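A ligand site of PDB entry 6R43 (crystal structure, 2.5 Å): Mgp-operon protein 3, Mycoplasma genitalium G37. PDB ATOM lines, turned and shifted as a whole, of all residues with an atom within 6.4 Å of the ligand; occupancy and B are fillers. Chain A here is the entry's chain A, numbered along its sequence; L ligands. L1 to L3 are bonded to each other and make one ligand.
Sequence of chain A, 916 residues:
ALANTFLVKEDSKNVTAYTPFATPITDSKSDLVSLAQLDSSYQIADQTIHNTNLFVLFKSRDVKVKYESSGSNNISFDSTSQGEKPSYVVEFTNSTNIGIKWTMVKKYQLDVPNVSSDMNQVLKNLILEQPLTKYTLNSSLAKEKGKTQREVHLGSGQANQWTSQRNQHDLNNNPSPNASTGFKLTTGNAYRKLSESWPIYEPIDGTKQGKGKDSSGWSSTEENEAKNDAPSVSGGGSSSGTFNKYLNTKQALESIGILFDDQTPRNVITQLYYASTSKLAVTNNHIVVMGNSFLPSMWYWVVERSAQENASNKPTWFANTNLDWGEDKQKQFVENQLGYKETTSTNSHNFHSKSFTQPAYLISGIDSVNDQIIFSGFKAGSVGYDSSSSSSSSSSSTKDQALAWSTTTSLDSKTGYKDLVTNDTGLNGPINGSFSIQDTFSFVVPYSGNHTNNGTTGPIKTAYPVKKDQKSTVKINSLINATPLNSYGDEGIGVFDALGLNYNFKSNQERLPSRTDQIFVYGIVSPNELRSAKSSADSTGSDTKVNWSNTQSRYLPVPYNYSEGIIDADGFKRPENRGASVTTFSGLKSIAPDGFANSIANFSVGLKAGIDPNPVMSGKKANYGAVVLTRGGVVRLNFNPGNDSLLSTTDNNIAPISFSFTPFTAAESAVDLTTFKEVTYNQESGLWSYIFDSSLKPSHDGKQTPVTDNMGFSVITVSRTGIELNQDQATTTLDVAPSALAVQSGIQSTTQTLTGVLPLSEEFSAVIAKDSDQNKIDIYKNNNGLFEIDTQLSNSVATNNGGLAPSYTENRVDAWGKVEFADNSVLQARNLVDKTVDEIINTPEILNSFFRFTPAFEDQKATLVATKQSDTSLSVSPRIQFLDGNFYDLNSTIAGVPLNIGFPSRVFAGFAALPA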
ATOM      1  N   ARG A 150      14.560 -20.037  -7.029  1.00  0.00           N
ATOM      2  CA  ARG A 150      13.331 -20.848  -7.139  1.00  0.00           C
ATOM      3  C   ARG A 150      13.259 -21.939  -6.055  1.00  0.00           C
ATOM      4  O   ARG A 150      12.114 -22.456  -5.822  1.00  0.00           O
ATOM      5  CB  ARG A 150      13.187 -21.322  -8.595  1.00  0.00           C
ATOM      6  CG  ARG A 150      13.525 -22.781  -8.868  1.00  0.00           C
ATOM      7  CD  ARG A 150      12.309 -23.714  -9.001  1.00  0.00           C
ATOM      8  NE  ARG A 150      12.691 -25.019  -8.486  1.00  0.00           N
ATOM      9  CZ  ARG A 150      13.760 -25.717  -8.880  1.00  0.00           C
ATOM     10  NH1 ARG A 150      14.545 -25.266  -9.857  1.00  0.00           N
ATOM     11  NH2 ARG A 150      14.046 -26.862  -8.318  1.00  0.00           N
ATOM     12  N   GLN A 158       9.760 -27.936  -8.239  1.00  0.00           N
ATOM     13  CA  GLN A 158      10.048 -27.984  -9.700  1.00  0.00           C
ATOM     14  C   GLN A 158      10.031 -26.583 -10.318  1.00  0.00           C
ATOM     15  O   GLN A 158       9.356 -25.680  -9.760  1.00  0.00           O
ATOM     16  CB  GLN A 158       9.073 -28.960 -10.378  1.00  0.00           C
ATOM     17  CG  GLN A 158       7.754 -29.122  -9.639  1.00  0.00           C
ATOM     18  CD  GLN A 158       6.643 -29.660 -10.507  1.00  0.00           C
ATOM     19  OE1 GLN A 158       6.763 -30.723 -11.113  1.00  0.00           O
ATOM     20  NE2 GLN A 158       5.545 -28.929 -10.552  1.00  0.00           N
ATOM     21  N   ALA A 159      10.757 -26.451 -11.437  1.00  0.00           N
ATOM     22  CA  ALA A 159      10.798 -25.289 -12.364  1.00  0.00           C
ATOM     23  C   ALA A 159       9.879 -25.566 -13.563  1.00  0.00           C
ATOM     24  O   ALA A 159       9.966 -24.863 -14.585  1.00  0.00           O
ATOM     25  CB  ALA A 159      12.233 -25.013 -12.784  1.00  0.00           C
ATOM     26  N   ASN A 160       9.038 -26.584 -13.433  1.00  0.00           N
ATOM     27  CA  ASN A 160       7.866 -26.827 -14.309  1.00  0.00           C
ATOM     28  C   ASN A 160       6.738 -25.877 -13.863  1.00  0.00           C
ATOM     29  O   ASN A 160       5.856 -25.588 -14.689  1.00  0.00           O
ATOM     30  CB  ASN A 160       7.475 -28.300 -14.262  1.00  0.00           C
ATOM     31  CG  ASN A 160       8.521 -29.211 -14.878  1.00  0.00           C
ATOM     32  OD1 ASN A 160       8.156 -30.111 -15.642  1.00  0.00           O
ATOM     33  ND2 ASN A 160       9.795 -28.999 -14.575  1.00  0.00           N
ATOM     34  N   TRP A 162       7.614 -22.841 -12.313  1.00  0.00           N
ATOM     35  CA  TRP A 162       8.328 -21.547 -12.191  1.00  0.00           C
ATOM     36  C   TRP A 162       7.523 -20.422 -12.827  1.00  0.00           C
ATOM     37  O   TRP A 162       7.545 -19.295 -12.301  1.00  0.00           O
ATOM     38  CB  TRP A 162       9.722 -21.615 -12.817  1.00  0.00           C
ATOM     39  CG  TRP A 162      10.447 -20.298 -12.860  1.00  0.00           C
ATOM     40  CD1 TRP A 162      10.840 -19.624 -13.982  1.00  0.00           C
ATOM     41  CD2 TRP A 162      10.867 -19.492 -11.747  1.00  0.00           C
ATOM     42  NE1 TRP A 162      11.476 -18.456 -13.647  1.00  0.00           N
ATOM     43  CE2 TRP A 162      11.514 -18.341 -12.280  1.00  0.00           C
ATOM     44  CE3 TRP A 162      10.772 -19.615 -10.350  1.00  0.00           C
ATOM     45  CZ2 TRP A 162      12.060 -17.350 -11.475  1.00  0.00           C
ATOM     46  CZ3 TRP A 162      11.306 -18.636  -9.560  1.00  0.00           C
ATOM     47  CH2 TRP A 162      11.950 -17.517 -10.110  1.00  0.00           C
ATOM     48  N   PRO A 175      13.452 -14.761 -15.733  1.00  0.00           N
ATOM     49  CA  PRO A 175      13.908 -15.946 -16.461  1.00  0.00           C
ATOM     50  C   PRO A 175      14.983 -16.783 -15.749  1.00  0.00           C
ATOM     51  O   PRO A 175      15.609 -17.613 -16.399  1.00  0.00           O
ATOM     52  CB  PRO A 175      14.482 -15.279 -17.735  1.00  0.00           C
ATOM     53  CG  PRO A 175      15.106 -13.991 -17.233  1.00  0.00           C
ATOM     54  CD  PRO A 175      14.200 -13.540 -16.108  1.00  0.00           C
ATOM     55  N   SER A 176      15.177 -16.580 -14.439  1.00  0.00           N
ATOM     56  CA  SER A 176      16.375 -17.000 -13.677  1.00  0.00           C
ATOM     57  C   SER A 176      15.979 -17.755 -12.412  1.00  0.00           C
ATOM     58  O   SER A 176      16.251 -17.298 -11.294  1.00  0.00           O
ATOM     59  CB  SER A 176      17.216 -15.793 -13.376  1.00  0.00           C
ATOM     60  OG  SER A 176      17.343 -14.964 -14.519  1.00  0.00           O
ATOM     61  N   PRO A 177      15.316 -18.924 -12.556  1.00  0.00           N
ATOM     62  CA  PRO A 177      14.978 -19.766 -11.410  1.00  0.00           C
ATOM     63  C   PRO A 177      16.221 -20.321 -10.706  1.00  0.00           C
ATOM     64  O   PRO A 177      16.122 -20.667  -9.549  1.00  0.00           O
ATOM     65  CB  PRO A 177      14.135 -20.899 -12.005  1.00  0.00           C
ATOM     66  CG  PRO A 177      14.520 -20.938 -13.472  1.00  0.00           C
ATOM     67  CD  PRO A 177      14.844 -19.506 -13.822  1.00  0.00           C
ATOM     68  N   ASN A 178      17.357 -20.372 -11.427  1.00  0.00           N
ATOM     69  CA  ASN A 178      18.645 -20.962 -10.971  1.00  0.00           C
ATOM     70  C   ASN A 178      19.709 -19.869 -10.804  1.00  0.00           C
ATOM     71  O   ASN A 178      20.937 -20.185 -10.798  1.00  0.00           O
ATOM     72  CB  ASN A 178      19.120 -22.067 -11.924  1.00  0.00           C
ATOM     73  CG  ASN A 178      17.986 -22.928 -12.450  1.00  0.00           C
ATOM     74  OD1 ASN A 178      17.195 -23.467 -11.676  1.00  0.00           O
ATOM     75  ND2 ASN A 178      17.931 -23.060 -13.759  1.00  0.00           N
ATOM     76  N   ALA A 179      19.282 -18.603 -10.712  1.00  0.00           N
ATOM     77  CA  ALA A 179      20.153 -17.520 -10.199  1.00  0.00           C
ATOM     78  C   ALA A 179      20.465 -17.865  -8.753  1.00  0.00           C
ATOM     79  O   ALA A 179      19.608 -18.491  -8.079  1.00  0.00           O
ATOM     80  CB  ALA A 179      19.527 -16.155 -10.332  1.00  0.00           C
ATOM     81  N   ILE A 431      19.188 -12.500 -10.655  1.00  0.00           N
ATOM     82  CA  ILE A 431      18.826 -12.463 -12.100  1.00  0.00           C
ATOM     83  C   ILE A 431      19.903 -13.166 -12.949  1.00  0.00           C
ATOM     84  O   ILE A 431      19.608 -13.492 -14.113  1.00  0.00           O
ATOM     85  CB  ILE A 431      18.572 -11.009 -12.531  1.00  0.00           C
ATOM     86  CG1 ILE A 431      17.459 -10.920 -13.588  1.00  0.00           C
ATOM     87  CG2 ILE A 431      19.839 -10.326 -12.981  1.00  0.00           C
ATOM     88  CD1 ILE A 431      17.166  -9.494 -14.074  1.00  0.00           C
ATOM     89  N   ASN A 432      21.104 -13.401 -12.411  1.00  0.00           N
ATOM     90  CA  ASN A 432      22.317 -13.808 -13.169  1.00  0.00           C
ATOM     91  C   ASN A 432      22.797 -15.211 -12.738  1.00  0.00           C
ATOM     92  O   ASN A 432      22.749 -15.570 -11.511  1.00  0.00           O
ATOM     93  CB  ASN A 432      23.383 -12.716 -13.053  1.00  0.00           C
ATOM     94  CG  ASN A 432      23.137 -11.555 -13.986  1.00  0.00           C
ATOM     95  OD1 ASN A 432      22.477 -11.729 -15.020  1.00  0.00           O
ATOM     96  ND2 ASN A 432      23.676 -10.381 -13.664  1.00  0.00           N
ATOM     97  N   GLY A 433      23.274 -15.978 -13.725  1.00  0.00           N
ATOM     98  CA  GLY A 433      23.775 -17.349 -13.552  1.00  0.00           C
ATOM     99  C   GLY A 433      24.378 -17.855 -14.839  1.00  0.00           C
ATOM    100  O   GLY A 433      25.510 -17.493 -15.102  1.00  0.00           O
ATOM    101  N   SER A 434      23.633 -18.638 -15.618  1.00  0.00           N
ATOM    102  CA  SER A 434      24.090 -19.252 -16.901  1.00  0.00           C
ATOM    103  C   SER A 434      22.925 -19.349 -17.899  1.00  0.00           C
ATOM    104  O   SER A 434      21.814 -19.727 -17.497  1.00  0.00           O
ATOM    105  CB  SER A 434      24.738 -20.585 -16.646  1.00  0.00           C
ATOM    106  OG  SER A 434      23.862 -21.411 -15.884  1.00  0.00           O
ATOM    107  N   PHE A 435      23.220 -19.032 -19.168  1.00  0.00           N
ATOM    108  CA  PHE A 435      22.249 -18.786 -20.273  1.00  0.00           C
ATOM    109  C   PHE A 435      22.847 -19.255 -21.598  1.00  0.00           C
ATOM    110  O   PHE A 435      23.776 -18.582 -22.119  1.00  0.00           O
ATOM    111  CB  PHE A 435      21.928 -17.296 -20.381  1.00  0.00           C
ATOM    112  CG  PHE A 435      21.287 -16.684 -19.162  1.00  0.00           C
ATOM    113  CD1 PHE A 435      20.037 -17.079 -18.748  1.00  0.00           C
ATOM    114  CD2 PHE A 435      21.925 -15.679 -18.457  1.00  0.00           C
ATOM    115  CE1 PHE A 435      19.429 -16.498 -17.639  1.00  0.00           C
ATOM    116  CE2 PHE A 435      21.305 -15.104 -17.347  1.00  0.00           C
ATOM    117  CZ  PHE A 435      20.060 -15.516 -16.950  1.00  0.00           C
ATOM    118  N   SER A 436      22.311 -20.352 -22.156  1.00  0.00           N
ATOM    119  CA  SER A 436      22.593 -20.837 -23.528  1.00  0.00           C
ATOM    120  C   SER A 436      21.407 -20.497 -24.437  1.00  0.00           C
ATOM    121  O   SER A 436      20.498 -21.346 -24.616  1.00  0.00           O
ATOM    122  CB  SER A 436      22.943 -22.295 -23.529  1.00  0.00           C
ATOM    123  OG  SER A 436      22.291 -22.958 -22.466  1.00  0.00           O
ATOM    124  N   ILE A 437      21.403 -19.254 -24.938  1.00  0.00           N
ATOM    125  CA  ILE A 437      20.622 -18.770 -26.124  1.00  0.00           C
ATOM    126  C   ILE A 437      21.193 -19.461 -27.377  1.00  0.00           C
ATOM    127  O   ILE A 437      22.437 -19.460 -27.510  1.00  0.00           O
ATOM    128  CB  ILE A 437      20.669 -17.221 -26.246  1.00  0.00           C
ATOM    129  CG1 ILE A 437      20.618 -16.731 -27.702  1.00  0.00           C
ATOM    130  CG2 ILE A 437      21.863 -16.603 -25.504  1.00  0.00           C
ATOM    131  CD1 ILE A 437      21.973 -16.510 -28.376  1.00  0.00           C
ATOM    132  N   PHE A 441      26.857 -18.972 -25.149  1.00  0.00           N
ATOM    133  CA  PHE A 441      26.842 -19.009 -23.668  1.00  0.00           C
ATOM    134  C   PHE A 441      27.018 -17.584 -23.154  1.00  0.00           C
ATOM    135  O   PHE A 441      27.659 -16.752 -23.829  1.00  0.00           O
ATOM    136  CB  PHE A 441      27.934 -19.936 -23.090  1.00  0.00           C
ATOM    137  CG  PHE A 441      27.633 -20.555 -21.746  1.00  0.00           C
ATOM    138  CD1 PHE A 441      27.692 -19.800 -20.583  1.00  0.00           C
ATOM    139  CD2 PHE A 441      27.338 -21.912 -21.629  1.00  0.00           C
ATOM    140  CE1 PHE A 441      27.425 -20.376 -19.340  1.00  0.00           C
ATOM    141  CE2 PHE A 441      27.092 -22.488 -20.396  1.00  0.00           C
ATOM    142  CZ  PHE A 441      27.121 -21.721 -19.249  1.00  0.00           C
ATOM    143  N   PHE A 443      26.726 -15.597 -18.856  1.00  0.00           N
ATOM    144  CA  PHE A 443      26.398 -15.619 -17.404  1.00  0.00           C
ATOM    145  C   PHE A 443      25.362 -14.554 -17.075  1.00  0.00           C
ATOM    146  O   PHE A 443      24.634 -14.689 -16.064  1.00  0.00           O
ATOM    147  CB  PHE A 443      27.649 -15.369 -16.561  1.00  0.00           C
ATOM    148  CG  PHE A 443      28.741 -16.383 -16.735  1.00  0.00           C
ATOM    149  CD1 PHE A 443      28.648 -17.636 -16.162  1.00  0.00           C
ATOM    150  CD2 PHE A 443      29.867 -16.069 -17.485  1.00  0.00           C
ATOM    151  CE1 PHE A 443      29.656 -18.565 -16.328  1.00  0.00           C
ATOM    152  CE2 PHE A 443      30.883 -16.997 -17.644  1.00  0.00           C
ATOM    153  CZ  PHE A 443      30.774 -18.246 -17.069  1.00  0.00           C
ATOM    154  N   PRO A 446      20.277 -12.005 -20.967  1.00  0.00           N
ATOM    155  CA  PRO A 446      20.413 -11.475 -22.325  1.00  0.00           C
ATOM    156  C   PRO A 446      19.533 -10.256 -22.615  1.00  0.00           C
ATOM    157  O   PRO A 446      19.818  -9.594 -23.621  1.00  0.00           O
ATOM    158  CB  PRO A 446      20.044 -12.660 -23.228  1.00  0.00           C
ATOM    159  CG  PRO A 446      19.925 -13.856 -22.293  1.00  0.00           C
ATOM    160  CD  PRO A 446      19.564 -13.281 -20.935  1.00  0.00           C
ATOM    161  N   TYR A 447      18.543  -9.959 -21.752  1.00  0.00           N
ATOM    162  CA  TYR A 447      17.571  -8.829 -21.887  1.00  0.00           C
ATOM    163  C   TYR A 447      17.049  -8.394 -20.498  1.00  0.00           C
ATOM    164  O   TYR A 447      16.836  -9.274 -19.649  1.00  0.00           O
ATOM    165  CB  TYR A 447      16.406  -9.205 -22.807  1.00  0.00           C
ATOM    166  CG  TYR A 447      16.265 -10.684 -23.059  1.00  0.00           C
ATOM    167  CD1 TYR A 447      16.057 -11.563 -22.010  1.00  0.00           C
ATOM    168  CD2 TYR A 447      16.359 -11.198 -24.340  1.00  0.00           C
ATOM    169  CE1 TYR A 447      15.951 -12.935 -22.226  1.00  0.00           C
ATOM    170  CE2 TYR A 447      16.245 -12.558 -24.583  1.00  0.00           C
ATOM    171  CZ  TYR A 447      16.040 -13.426 -23.526  1.00  0.00           C
ATOM    172  OH  TYR A 447      15.922 -14.756 -23.757  1.00  0.00           O
HETATM  173  C1  LIG L   1      14.986 -25.927 -16.254  1.00  0.00           C
HETATM  174  C2  LIG L   1      16.123 -26.013 -17.266  1.00  0.00           C
HETATM  175  C3  LIG L   1      15.915 -27.160 -18.248  1.00  0.00           C
HETATM  176  C4  LIG L   1      15.068 -28.325 -17.679  1.00  0.00           C
HETATM  177  C5  LIG L   1      15.799 -29.102 -16.576  1.00  0.00           C
HETATM  178  C6  LIG L   1      13.683 -26.425 -16.937  1.00  0.00           C
HETATM  179  O1  LIG L   1      12.508 -26.135 -16.169  1.00  0.00           O
HETATM  180  O2  LIG L   1      14.902 -24.579 -15.738  1.00  0.00           O
HETATM  181  O3  LIG L   1      17.345 -26.229 -16.601  1.00  0.00           O
HETATM  182  O4  LIG L   1      15.197 -26.628 -19.367  1.00  0.00           O
HETATM  183  O5  LIG L   1      13.773 -27.854 -17.226  1.00  0.00           O
HETATM  184  O6  LIG L   1      15.702 -30.505 -16.840  1.00  0.00           O
HETATM  185  C1  LG2 L   2      15.918 -26.525 -20.582  1.00  0.00           C
HETATM  186  C2  LG2 L   2      14.931 -26.261 -21.703  1.00  0.00           C
HETATM  187  C3  LG2 L   2      15.712 -26.634 -22.945  1.00  0.00           C
HETATM  188  C4  LG2 L   2      16.776 -25.548 -23.109  1.00  0.00           C
HETATM  189  C5  LG2 L   2      17.499 -25.114 -21.776  1.00  0.00           C
HETATM  190  C6  LG2 L   2      17.751 -23.628 -21.547  1.00  0.00           C
HETATM  191  O1  LG2 L   2      13.700 -26.980 -21.587  1.00  0.00           O
HETATM  192  O2  LG2 L   2      14.812 -26.776 -24.053  1.00  0.00           O
HETATM  193  O3  LG2 L   2      16.101 -24.482 -23.786  1.00  0.00           O
HETATM  194  O4  LG2 L   2      16.873 -25.458 -20.530  1.00  0.00           O
HETATM  195  O5  LG2 L   2      18.038 -23.612 -20.143  1.00  0.00           O
HETATM  196  C1  LG3 L   3      19.865 -21.963 -20.355  1.00  0.00           C
HETATM  197  C2  LG3 L   3      18.777 -22.566 -19.492  1.00  0.00           C
HETATM  198  C3  LG3 L   3      19.337 -23.155 -18.183  1.00  0.00           C
HETATM  199  C4  LG3 L   3      19.739 -22.100 -17.148  1.00  0.00           C
HETATM  200  C5  LG3 L   3      18.675 -21.042 -16.909  1.00  0.00           C
HETATM  201  C6  LG3 L   3      18.210 -20.539 -18.256  1.00  0.00           C
HETATM  202  C7  LG3 L   3      17.015 -19.596 -18.111  1.00  0.00           C
HETATM  203  C8  LG3 L   3      16.698 -19.087 -19.510  1.00  0.00           C
HETATM  204  C9  LG3 L   3      15.977 -17.748 -19.472  1.00  0.00           C
HETATM  205  C10 LG3 L   3      18.865 -19.489 -14.972  1.00  0.00           C
HETATM  206  C11 LG3 L   3      19.640 -18.266 -14.487  1.00  0.00           C
HETATM  207  N1  LG3 L   3      19.227 -19.911 -16.191  1.00  0.00           N
HETATM  208  O1  LG3 L   3      19.625 -21.005 -21.118  1.00  0.00           O
HETATM  209  O2  LG3 L   3      21.011 -22.419 -20.316  1.00  0.00           O
HETATM  210  O3  LG3 L   3      20.034 -22.715 -15.894  1.00  0.00           O
HETATM  211  O4  LG3 L   3      17.817 -21.582 -19.148  1.00  0.00           O
HETATM  212  O5  LG3 L   3      15.851 -20.229 -17.513  1.00  0.00           O
HETATM  213  O6  LG3 L   3      17.925 -18.936 -20.214  1.00  0.00           O
HETATM  214  O7  LG3 L   3      15.467 -17.427 -20.768  1.00  0.00           O
HETATM  215  O8  LG3 L   3      18.004 -20.018 -14.294  1.00  0.00           O
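An oxygen (O8) of LG3 L3 lies close to the backbone nitrogen (N) of Pro 177 (3.4 Å).
Ser 176 touches the ligand.
Ala 179 touches the ligand.
CD1 of Phe 435 touches O6 of LG3 L3 (3.2 Å).
Within 4 Å of the ligand: Ala 159, Pro 175, Ser 176, Pro 177, Asn 178, Ala 179, Ser 434, Phe 435 and Ser 436.
The nearest printed residue that does not touch the ligand is Tyr 447 (4.03 Å).
O of Ala 159 is in hydrogen-bond range of O1 of LIG L1, 3.3 Å away.
N1 of LG3 L3 lies within hydrogen-bond range of O of Ser 434 (2.9 Å).
The backbone NH (N) of Ser 436 lies within hydrogen-bond range of an oxygen (O1) of LG3 L3 (3.0 Å).
The backbone NH of Asn 178 lies within hydrogen-bond range of an oxygen (O8) of LG3 L3.
O of Pro 175 sits at hydrogen-bond distance from O5 of LG3 L3 (2.9 Å).
The side-chain amide nitrogen (ND2) of Asn 178 is in hydrogen-bond range of an oxygen (O3) of LG3 L3.
O2 of LG3 L3 is in hydrogen-bond range of OG of Ser 436 (2.6 Å).
The backbone carbonyl oxygen of Pro 177 lies within hydrogen-bond range of the backbone NH of Arg 150, 3.0 Å away.
The backbone carbonyl oxygen (O) of Ile 431 lies within hydrogen-bond range of the side-chain hydroxyl (OG) of Ser 176, 2.7 Å away.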
